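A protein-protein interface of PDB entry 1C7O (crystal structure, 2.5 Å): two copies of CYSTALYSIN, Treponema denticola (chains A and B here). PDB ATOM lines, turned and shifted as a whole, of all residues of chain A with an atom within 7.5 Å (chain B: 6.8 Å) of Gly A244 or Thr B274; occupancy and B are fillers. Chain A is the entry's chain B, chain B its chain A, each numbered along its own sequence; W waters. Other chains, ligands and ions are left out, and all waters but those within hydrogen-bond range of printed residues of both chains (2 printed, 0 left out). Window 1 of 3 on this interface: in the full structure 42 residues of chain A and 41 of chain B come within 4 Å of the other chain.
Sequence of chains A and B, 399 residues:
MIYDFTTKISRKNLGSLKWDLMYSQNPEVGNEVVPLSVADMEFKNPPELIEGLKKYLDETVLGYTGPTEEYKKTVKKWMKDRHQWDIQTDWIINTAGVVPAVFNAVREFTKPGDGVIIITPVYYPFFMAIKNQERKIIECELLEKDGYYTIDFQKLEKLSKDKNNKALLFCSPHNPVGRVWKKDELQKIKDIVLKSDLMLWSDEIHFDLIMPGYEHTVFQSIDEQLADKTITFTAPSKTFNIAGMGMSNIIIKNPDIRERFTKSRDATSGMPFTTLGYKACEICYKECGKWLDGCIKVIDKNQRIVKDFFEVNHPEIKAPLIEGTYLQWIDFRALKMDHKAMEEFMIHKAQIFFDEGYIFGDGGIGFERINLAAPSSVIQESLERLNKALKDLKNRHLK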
ATOM      1  N   ASP A  40       0.409   9.063 -27.299  1.00  0.00           N
ATOM      2  CA  ASP A  40       0.294  10.078 -26.267  1.00  0.00           C
ATOM      3  C   ASP A  40       1.277  11.133 -26.757  1.00  0.00           C
ATOM      4  O   ASP A  40       2.187  10.824 -27.529  1.00  0.00           O
ATOM      5  CB  ASP A  40       0.577   9.528 -24.852  1.00  0.00           C
ATOM      6  CG  ASP A  40       2.028   9.177 -24.598  1.00  0.00           C
ATOM      7  OD1 ASP A  40       2.286   8.577 -23.529  1.00  0.00           O
ATOM      8  OD2 ASP A  40       2.903   9.494 -25.424  1.00  0.00           O
ATOM      9  N   ALA A  96     -12.723   3.768 -16.927  1.00  0.00           N
ATOM     10  CA  ALA A  96     -11.361   4.274 -16.774  1.00  0.00           C
ATOM     11  C   ALA A  96     -10.672   4.478 -18.111  1.00  0.00           C
ATOM     12  O   ALA A  96      -9.672   5.187 -18.199  1.00  0.00           O
ATOM     13  CB  ALA A  96     -10.549   3.331 -15.917  1.00  0.00           C
ATOM     14  N   SER A 237      -8.761  12.103 -23.263  1.00  0.00           N
ATOM     15  CA  SER A 237      -7.396  11.608 -23.123  1.00  0.00           C
ATOM     16  C   SER A 237      -6.523  11.891 -24.335  1.00  0.00           C
ATOM     17  O   SER A 237      -5.441  12.466 -24.204  1.00  0.00           O
ATOM     18  CB  SER A 237      -7.430  10.113 -22.819  1.00  0.00           C
ATOM     19  OG  SER A 237      -8.324   9.451 -23.699  1.00  0.00           O
ATOM     20  N   ASN A 241      -3.947  14.940 -24.156  1.00  0.00           N
ATOM     21  CA  ASN A 241      -2.811  14.202 -23.640  1.00  0.00           C
ATOM     22  C   ASN A 241      -2.954  13.757 -22.189  1.00  0.00           C
ATOM     23  O   ASN A 241      -1.987  13.815 -21.414  1.00  0.00           O
ATOM     24  CB  ASN A 241      -1.543  15.051 -23.795  1.00  0.00           C
ATOM     25  CG  ASN A 241      -0.283  14.208 -23.831  1.00  0.00           C
ATOM     26  OD1 ASN A 241      -0.339  12.997 -24.082  1.00  0.00           O
ATOM     27  ND2 ASN A 241       0.864  14.844 -23.599  1.00  0.00           N
ATOM     28  N   ILE A 242      -4.146  13.291 -21.824  1.00  0.00           N
ATOM     29  CA  ILE A 242      -4.374  12.844 -20.457  1.00  0.00           C
ATOM     30  C   ILE A 242      -4.797  11.384 -20.316  1.00  0.00           C
ATOM     31  O   ILE A 242      -5.680  11.063 -19.515  1.00  0.00           O
ATOM     32  CB  ILE A 242      -5.416  13.744 -19.733  1.00  0.00           C
ATOM     33  CG1 ILE A 242      -6.752  13.724 -20.472  1.00  0.00           C
ATOM     34  CG2 ILE A 242      -4.888  15.167 -19.631  1.00  0.00           C
ATOM     35  CD1 ILE A 242      -7.859  14.504 -19.755  1.00  0.00           C
ATOM     36  N   ALA A 243      -4.159  10.499 -21.083  1.00  0.00           N
ATOM     37  CA  ALA A 243      -4.446   9.067 -21.010  1.00  0.00           C
ATOM     38  C   ALA A 243      -4.027   8.532 -19.636  1.00  0.00           C
ATOM     39  O   ALA A 243      -4.308   7.373 -19.293  1.00  0.00           O
ATOM     40  CB  ALA A 243      -3.699   8.328 -22.096  1.00  0.00           C
ATOM     41  N   GLY A 244      -3.348   9.379 -18.861  1.00  0.00           N
ATOM     42  CA  GLY A 244      -2.907   9.001 -17.530  1.00  0.00           C
ATOM     43  C   GLY A 244      -3.859   9.441 -16.424  1.00  0.00           C
ATOM     44  O   GLY A 244      -3.630   9.145 -15.249  1.00  0.00           O
ATOM     45  N   MET A 245      -4.928  10.147 -16.781  1.00  0.00           N
ATOM     46  CA  MET A 245      -5.894  10.600 -15.781  1.00  0.00           C
ATOM     47  C   MET A 245      -7.045   9.602 -15.593  1.00  0.00           C
ATOM     48  O   MET A 245      -7.838   9.710 -14.651  1.00  0.00           O
ATOM     49  CB  MET A 245      -6.431  11.984 -16.153  1.00  0.00           C
ATOM     50  CG  MET A 245      -5.388  13.098 -16.032  1.00  0.00           C
ATOM     51  SD  MET A 245      -4.619  13.170 -14.379  1.00  0.00           S
ATOM     52  CE  MET A 245      -5.869  14.009 -13.463  1.00  0.00           C
ATOM     53  N   GLY A 246      -7.123   8.634 -16.502  1.00  0.00           N
ATOM     54  CA  GLY A 246      -8.126   7.583 -16.434  1.00  0.00           C
ATOM     55  C   GLY A 246      -9.610   7.905 -16.397  1.00  0.00           C
ATOM     56  O   GLY A 246     -10.296   7.534 -15.439  1.00  0.00           O
ATOM     57  N   MET A 247     -10.120   8.561 -17.437  1.00  0.00           N
ATOM     58  CA  MET A 247     -11.541   8.892 -17.493  1.00  0.00           C
ATOM     59  C   MET A 247     -12.081   8.870 -18.923  1.00  0.00           C
ATOM     60  O   MET A 247     -11.451   9.378 -19.846  1.00  0.00           O
ATOM     61  CB  MET A 247     -11.783  10.264 -16.860  1.00  0.00           C
ATOM     62  CG  MET A 247     -13.248  10.662 -16.766  1.00  0.00           C
ATOM     63  SD  MET A 247     -14.282   9.391 -15.997  1.00  0.00           S
ATOM     64  CE  MET A 247     -13.486   9.198 -14.388  1.00  0.00           C
ATOM     65  N   THR A 274     -11.808   7.751  -9.369  1.00  0.00           N
ATOM     66  CA  THR A 274     -10.782   8.763  -9.560  1.00  0.00           C
ATOM     67  C   THR A 274     -11.371  10.153  -9.370  1.00  0.00           C
ATOM     68  O   THR A 274     -12.324  10.525 -10.035  1.00  0.00           O
ATOM     69  CB  THR A 274     -10.192   8.648 -10.985  1.00  0.00           C
ATOM     70  OG1 THR A 274      -9.322   9.753 -11.247  1.00  0.00           O
ATOM     71  CG2 THR A 274     -11.304   8.631 -12.009  1.00  0.00           C
ATOM     72  N   GLY A 277      -9.739  12.580 -12.198  1.00  0.00           N
ATOM     73  CA  GLY A 277     -10.068  12.144 -13.547  1.00  0.00           C
ATOM     74  C   GLY A 277     -11.216  12.968 -14.114  1.00  0.00           C
ATOM     75  O   GLY A 277     -11.117  13.496 -15.224  1.00  0.00           O
ATOM     76  N   VAL B  61       4.150  14.741 -17.494  1.00  0.00           N
ATOM     77  CA  VAL B  61       3.308  14.689 -18.681  1.00  0.00           C
ATOM     78  C   VAL B  61       2.302  13.600 -18.313  1.00  0.00           C
ATOM     79  O   VAL B  61       2.695  12.482 -17.980  1.00  0.00           O
ATOM     80  CB  VAL B  61       4.106  14.248 -19.933  1.00  0.00           C
ATOM     81  CG1 VAL B  61       3.159  13.957 -21.088  1.00  0.00           C
ATOM     82  CG2 VAL B  61       5.072  15.327 -20.334  1.00  0.00           C
ATOM     83  N   LEU B  62       1.012  13.915 -18.371  1.00  0.00           N
ATOM     84  CA  LEU B  62      -0.029  12.956 -17.987  1.00  0.00           C
ATOM     85  C   LEU B  62      -0.417  11.912 -19.046  1.00  0.00           C
ATOM     86  O   LEU B  62      -1.604  11.739 -19.358  1.00  0.00           O
ATOM     87  CB  LEU B  62      -1.267  13.732 -17.523  1.00  0.00           C
ATOM     88  CG  LEU B  62      -1.008  14.739 -16.390  1.00  0.00           C
ATOM     89  CD1 LEU B  62      -2.226  15.614 -16.177  1.00  0.00           C
ATOM     90  CD2 LEU B  62      -0.662  14.003 -15.115  1.00  0.00           C
ATOM     91  N   GLY B  63       0.577  11.199 -19.574  1.00  0.00           N
ATOM     92  CA  GLY B  63       0.315  10.189 -20.588  1.00  0.00           C
ATOM     93  C   GLY B  63       0.298   8.772 -20.046  1.00  0.00           C
ATOM     94  O   GLY B  63       0.204   8.573 -18.838  1.00  0.00           O
ATOM     95  N   TYR B  64       0.390   7.780 -20.930  1.00  0.00           N
ATOM     96  CA  TYR B  64       0.379   6.382 -20.493  1.00  0.00           C
ATOM     97  C   TYR B  64       1.525   6.106 -19.527  1.00  0.00           C
ATOM     98  O   TYR B  64       2.691   6.119 -19.913  1.00  0.00           O
ATOM     99  CB  TYR B  64       0.453   5.449 -21.706  1.00  0.00           C
ATOM    100  CG  TYR B  64      -0.834   5.422 -22.499  1.00  0.00           C
ATOM    101  CD1 TYR B  64      -1.986   4.847 -21.968  1.00  0.00           C
ATOM    102  CD2 TYR B  64      -0.923   6.043 -23.745  1.00  0.00           C
ATOM    103  CE1 TYR B  64      -3.202   4.894 -22.658  1.00  0.00           C
ATOM    104  CE2 TYR B  64      -2.132   6.101 -24.438  1.00  0.00           C
ATOM    105  CZ  TYR B  64      -3.269   5.527 -23.888  1.00  0.00           C
ATOM    106  OH  TYR B  64      -4.476   5.613 -24.554  1.00  0.00           O
ATOM    107  N   THR B  65       1.179   5.847 -18.268  1.00  0.00           N
ATOM    108  CA  THR B  65       2.175   5.608 -17.237  1.00  0.00           C
ATOM    109  C   THR B  65       2.040   4.258 -16.561  1.00  0.00           C
ATOM    110  O   THR B  65       0.935   3.738 -16.392  1.00  0.00           O
ATOM    111  CB  THR B  65       2.105   6.686 -16.123  1.00  0.00           C
ATOM    112  OG1 THR B  65       2.004   7.993 -16.705  1.00  0.00           O
ATOM    113  CG2 THR B  65       3.356   6.628 -15.259  1.00  0.00           C
ATOM    114  N   GLY B  66       3.185   3.706 -16.164  1.00  0.00           N
ATOM    115  CA  GLY B  66       3.229   2.432 -15.480  1.00  0.00           C
ATOM    116  C   GLY B  66       4.115   2.607 -14.262  1.00  0.00           C
ATOM    117  O   GLY B  66       4.705   3.672 -14.100  1.00  0.00           O
ATOM    118  N   ALA B  96      -6.833  -1.081 -10.565  1.00  0.00           N
ATOM    119  CA  ALA B  96      -7.468   0.170 -10.169  1.00  0.00           C
ATOM    120  C   ALA B  96      -7.985   0.092  -8.741  1.00  0.00           C
ATOM    121  O   ALA B  96      -7.787   1.019  -7.956  1.00  0.00           O
ATOM    122  CB  ALA B  96      -8.596   0.502 -11.105  1.00  0.00           C
ATOM    123  N   MET B 245      -7.560   7.909  -5.736  1.00  0.00           N
ATOM    124  CA  MET B 245      -6.340   7.949  -6.546  1.00  0.00           C
ATOM    125  C   MET B 245      -6.175   6.650  -7.333  1.00  0.00           C
ATOM    126  O   MET B 245      -5.274   6.509  -8.168  1.00  0.00           O
ATOM    127  CB  MET B 245      -5.112   8.208  -5.673  1.00  0.00           C
ATOM    128  CG  MET B 245      -4.979   9.670  -5.252  1.00  0.00           C
ATOM    129  SD  MET B 245      -4.748  10.836  -6.638  1.00  0.00           S
ATOM    130  CE  MET B 245      -3.075  11.330  -6.425  1.00  0.00           C
ATOM    131  N   GLY B 246      -7.074   5.712  -7.056  1.00  0.00           N
ATOM    132  CA  GLY B 246      -7.094   4.426  -7.735  1.00  0.00           C
ATOM    133  C   GLY B 246      -5.789   3.711  -8.032  1.00  0.00           C
ATOM    134  O   GLY B 246      -5.324   3.710  -9.177  1.00  0.00           O
ATOM    135  N   MET B 247      -5.195   3.097  -7.013  1.00  0.00           N
ATOM    136  CA  MET B 247      -3.968   2.347  -7.218  1.00  0.00           C
ATOM    137  C   MET B 247      -3.825   1.244  -6.197  1.00  0.00           C
ATOM    138  O   MET B 247      -3.567   1.505  -5.031  1.00  0.00           O
ATOM    139  CB  MET B 247      -2.741   3.247  -7.152  1.00  0.00           C
ATOM    140  CG  MET B 247      -1.467   2.507  -7.550  1.00  0.00           C
ATOM    141  SD  MET B 247      -1.720   1.573  -9.088  1.00  0.00           S
ATOM    142  CE  MET B 247      -1.503   2.871 -10.305  1.00  0.00           C
ATOM    143  N   MET B 271      -4.487  -2.856 -17.523  1.00  0.00           N
ATOM    144  CA  MET B 271      -3.488  -2.229 -16.667  1.00  0.00           C
ATOM    145  C   MET B 271      -3.852  -0.780 -16.361  1.00  0.00           C
ATOM    146  O   MET B 271      -4.347  -0.061 -17.230  1.00  0.00           O
ATOM    147  CB  MET B 271      -2.118  -2.267 -17.348  1.00  0.00           C
ATOM    148  CG  MET B 271      -0.966  -1.784 -16.475  1.00  0.00           C
ATOM    149  SD  MET B 271       0.526  -1.397 -17.427  1.00  0.00           S
ATOM    150  CE  MET B 271       0.858   0.302 -16.914  1.00  0.00           C
ATOM    151  N   PRO B 272      -3.621  -0.333 -15.119  1.00  0.00           N
ATOM    152  CA  PRO B 272      -3.933   1.047 -14.743  1.00  0.00           C
ATOM    153  C   PRO B 272      -2.826   1.941 -15.296  1.00  0.00           C
ATOM    154  O   PRO B 272      -1.647   1.626 -15.137  1.00  0.00           O
ATOM    155  CB  PRO B 272      -3.910   1.018 -13.208  1.00  0.00           C
ATOM    156  CG  PRO B 272      -4.035  -0.446 -12.859  1.00  0.00           C
ATOM    157  CD  PRO B 272      -3.228  -1.115 -13.934  1.00  0.00           C
ATOM    158  N   PHE B 273      -3.201   3.038 -15.944  1.00  0.00           N
ATOM    159  CA  PHE B 273      -2.221   3.966 -16.508  1.00  0.00           C
ATOM    160  C   PHE B 273      -2.208   5.283 -15.736  1.00  0.00           C
ATOM    161  O   PHE B 273      -1.441   6.193 -16.049  1.00  0.00           O
ATOM    162  CB  PHE B 273      -2.546   4.261 -17.970  1.00  0.00           C
ATOM    163  CG  PHE B 273      -2.523   3.053 -18.855  1.00  0.00           C
ATOM    164  CD1 PHE B 273      -3.632   2.720 -19.621  1.00  0.00           C
ATOM    165  CD2 PHE B 273      -1.386   2.251 -18.939  1.00  0.00           C
ATOM    166  CE1 PHE B 273      -3.616   1.608 -20.458  1.00  0.00           C
ATOM    167  CE2 PHE B 273      -1.360   1.133 -19.776  1.00  0.00           C
ATOM    168  CZ  PHE B 273      -2.476   0.810 -20.536  1.00  0.00           C
ATOM    169  N   THR B 274      -3.070   5.377 -14.732  1.00  0.00           N
ATOM    170  CA  THR B 274      -3.189   6.582 -13.922  1.00  0.00           C
ATOM    171  C   THR B 274      -1.860   7.015 -13.295  1.00  0.00           C
ATOM    172  O   THR B 274      -1.444   6.502 -12.252  1.00  0.00           O
ATOM    173  CB  THR B 274      -4.263   6.388 -12.825  1.00  0.00           C
ATOM    174  OG1 THR B 274      -4.175   7.450 -11.864  1.00  0.00           O
ATOM    175  CG2 THR B 274      -4.079   5.056 -12.139  1.00  0.00           C
ATOM    176  N   THR B 275      -1.210   7.975 -13.940  1.00  0.00           N
ATOM    177  CA  THR B 275       0.075   8.494 -13.492  1.00  0.00           C
ATOM    178  C   THR B 275       0.148   8.987 -12.039  1.00  0.00           C
ATOM    179  O   THR B 275       1.112   8.673 -11.329  1.00  0.00           O
ATOM    180  CB  THR B 275       0.545   9.621 -14.424  1.00  0.00           C
ATOM    181  OG1 THR B 275       1.684  10.284 -13.852  1.00  0.00           O
ATOM    182  CG2 THR B 275      -0.582  10.608 -14.660  1.00  0.00           C
ATOM    183  N   LEU B 276      -0.853   9.746 -11.592  1.00  0.00           N
ATOM    184  CA  LEU B 276      -0.855  10.261 -10.221  1.00  0.00           C
ATOM    185  C   LEU B 276      -1.068   9.159  -9.188  1.00  0.00           C
ATOM    186  O   LEU B 276      -0.562   9.243  -8.057  1.00  0.00           O
ATOM    187  CB  LEU B 276      -1.924  11.346 -10.049  1.00  0.00           C
ATOM    188  CG  LEU B 276      -1.770  12.574 -10.955  1.00  0.00           C
ATOM    189  CD1 LEU B 276      -2.912  13.535 -10.689  1.00  0.00           C
ATOM    190  CD2 LEU B 276      -0.440  13.251 -10.707  1.00  0.00           C
ATOM    191  N   GLY B 277      -1.813   8.125  -9.570  1.00  0.00           N
ATOM    192  CA  GLY B 277      -2.048   7.026  -8.651  1.00  0.00           C
ATOM    193  C   GLY B 277      -0.738   6.436  -8.156  1.00  0.00           C
ATOM    194  O   GLY B 277      -0.577   6.181  -6.964  1.00  0.00           O
ATOM    195  N   TYR B 278       0.208   6.222  -9.064  1.00  0.00           N
ATOM    196  CA  TYR B 278       1.498   5.657  -8.677  1.00  0.00           C
ATOM    197  C   TYR B 278       2.272   6.600  -7.762  1.00  0.00           C
ATOM    198  O   TYR B 278       2.853   6.170  -6.764  1.00  0.00           O
ATOM    199  CB  TYR B 278       2.356   5.345  -9.908  1.00  0.00           C
ATOM    200  CG  TYR B 278       1.805   4.270 -10.812  1.00  0.00           C
ATOM    201  CD1 TYR B 278       1.144   4.598 -11.989  1.00  0.00           C
ATOM    202  CD2 TYR B 278       1.963   2.925 -10.505  1.00  0.00           C
ATOM    203  CE1 TYR B 278       0.654   3.610 -12.845  1.00  0.00           C
ATOM    204  CE2 TYR B 278       1.476   1.928 -11.352  1.00  0.00           C
ATOM    205  CZ  TYR B 278       0.824   2.282 -12.520  1.00  0.00           C
ATOM    206  OH  TYR B 278       0.344   1.313 -13.371  1.00  0.00           O
ATOM    207  N   LYS B 279       2.271   7.884  -8.103  1.00  0.00           N
ATOM    208  CA  LYS B 279       2.977   8.892  -7.322  1.00  0.00           C
ATOM    209  C   LYS B 279       2.416   9.072  -5.905  1.00  0.00           C
ATOM    210  O   LYS B 279       3.171   9.212  -4.941  1.00  0.00           O
ATOM    211  CB  LYS B 279       2.947  10.231  -8.064  1.00  0.00           C
ATOM    212  CG  LYS B 279       3.877  11.270  -7.488  1.00  0.00           C
ATOM    213  CD  LYS B 279       5.315  10.778  -7.557  1.00  0.00           C
ATOM    214  CE  LYS B 279       6.308  11.861  -7.165  1.00  0.00           C
ATOM    215  NZ  LYS B 279       7.704  11.347  -7.258  1.00  0.00           N
HETATM  216  O   HOH W   1       3.716   6.708 -22.177  1.00  0.00           O
HETATM  217  O   HOH W   2      -7.608  11.190  -8.909  1.00  0.00           O
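Water W1 lies within hydrogen-bond range of O of Tyr B64 (2.6 Å) and OD1 of Asp A40 (2.7 Å).
Water W2 bridges the side-chain hydroxyl of Thr A274 and the side-chain sulfur of Met B245.
Among the printed residues, pairs that only touch across the chains: Gly A244 with Thr B274, Ile A242 with Leu B62, Ala A243 with Tyr B64, Gly A244 with Gly B63, Gly A244 with Phe B273, Asn A241 with Val B61, Ala A243 with Phe B273, Met A245 with Leu B62 and Asp A40 with Gly B63.
Hydrophobic or aromatic side chains of chain A that line the printed part of chain B: Ala A243 and Met A245.
Of the 19 printed residues of chain B, 7 touch a printed residue of chain A.
The backbone carbonyl oxygen of Gly B63 lies within hydrogen-bond range of the side-chain hydroxyl of Thr B65, at 2.9 Å.
The side-chain hydroxyl of Thr B274 is in hydrogen-bond range of the backbone NH of Gly B277 (3.4 Å).
The backbone NH (N) of Thr B65 is in hydrogen-bond range of the backbone carbonyl oxygen (O) of Phe B273 (3.5 Å).
O of Ser A237 is in hydrogen-bond range of N of Ile A242 (2.8 Å).
Positions printed for both chains: 96, 245, 246, 247, 274 and 277.
Of the printed residues of chain A, Leu B62 touches Asn A241, Ile A242, Ala A243, Gly A244 and Met A245.
Of the printed residues of chain A, Phe B273 touches Ala A243 (3.8 Å) and Gly A244 (3.5 Å).
Thr B274 touches one residue of chain A.
The nearest residue of chain B that does not touch Gly A244 is Tyr B64 (4.6 Å).
The nearest printed residue of chain B that does not touch Asp A40 is Val B61 (6.0 Å).
The backbone NH of Thr B275 is in hydrogen-bond range of the backbone carbonyl oxygen of Gly A244 (3.0 Å).
The backbone carbonyl oxygen (O) of Leu B62 sits at hydrogen-bond distance from the backbone NH (N) of Ala A243 (3.3 Å).
The backbone NH (N) of Tyr B64 sits at hydrogen-bond distance from the side-chain carboxylate (OD1) of Asp A40 (3.3 Å).
The backbone carbonyl oxygen (O) of Leu B62 sits at hydrogen-bond distance from the backbone NH (N) of Gly A244, at 3.0 Å.
The backbone carbonyl oxygen of Asn A241 lies close to the backbone carbonyl oxygen of Leu B62, 2.9 Å away.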
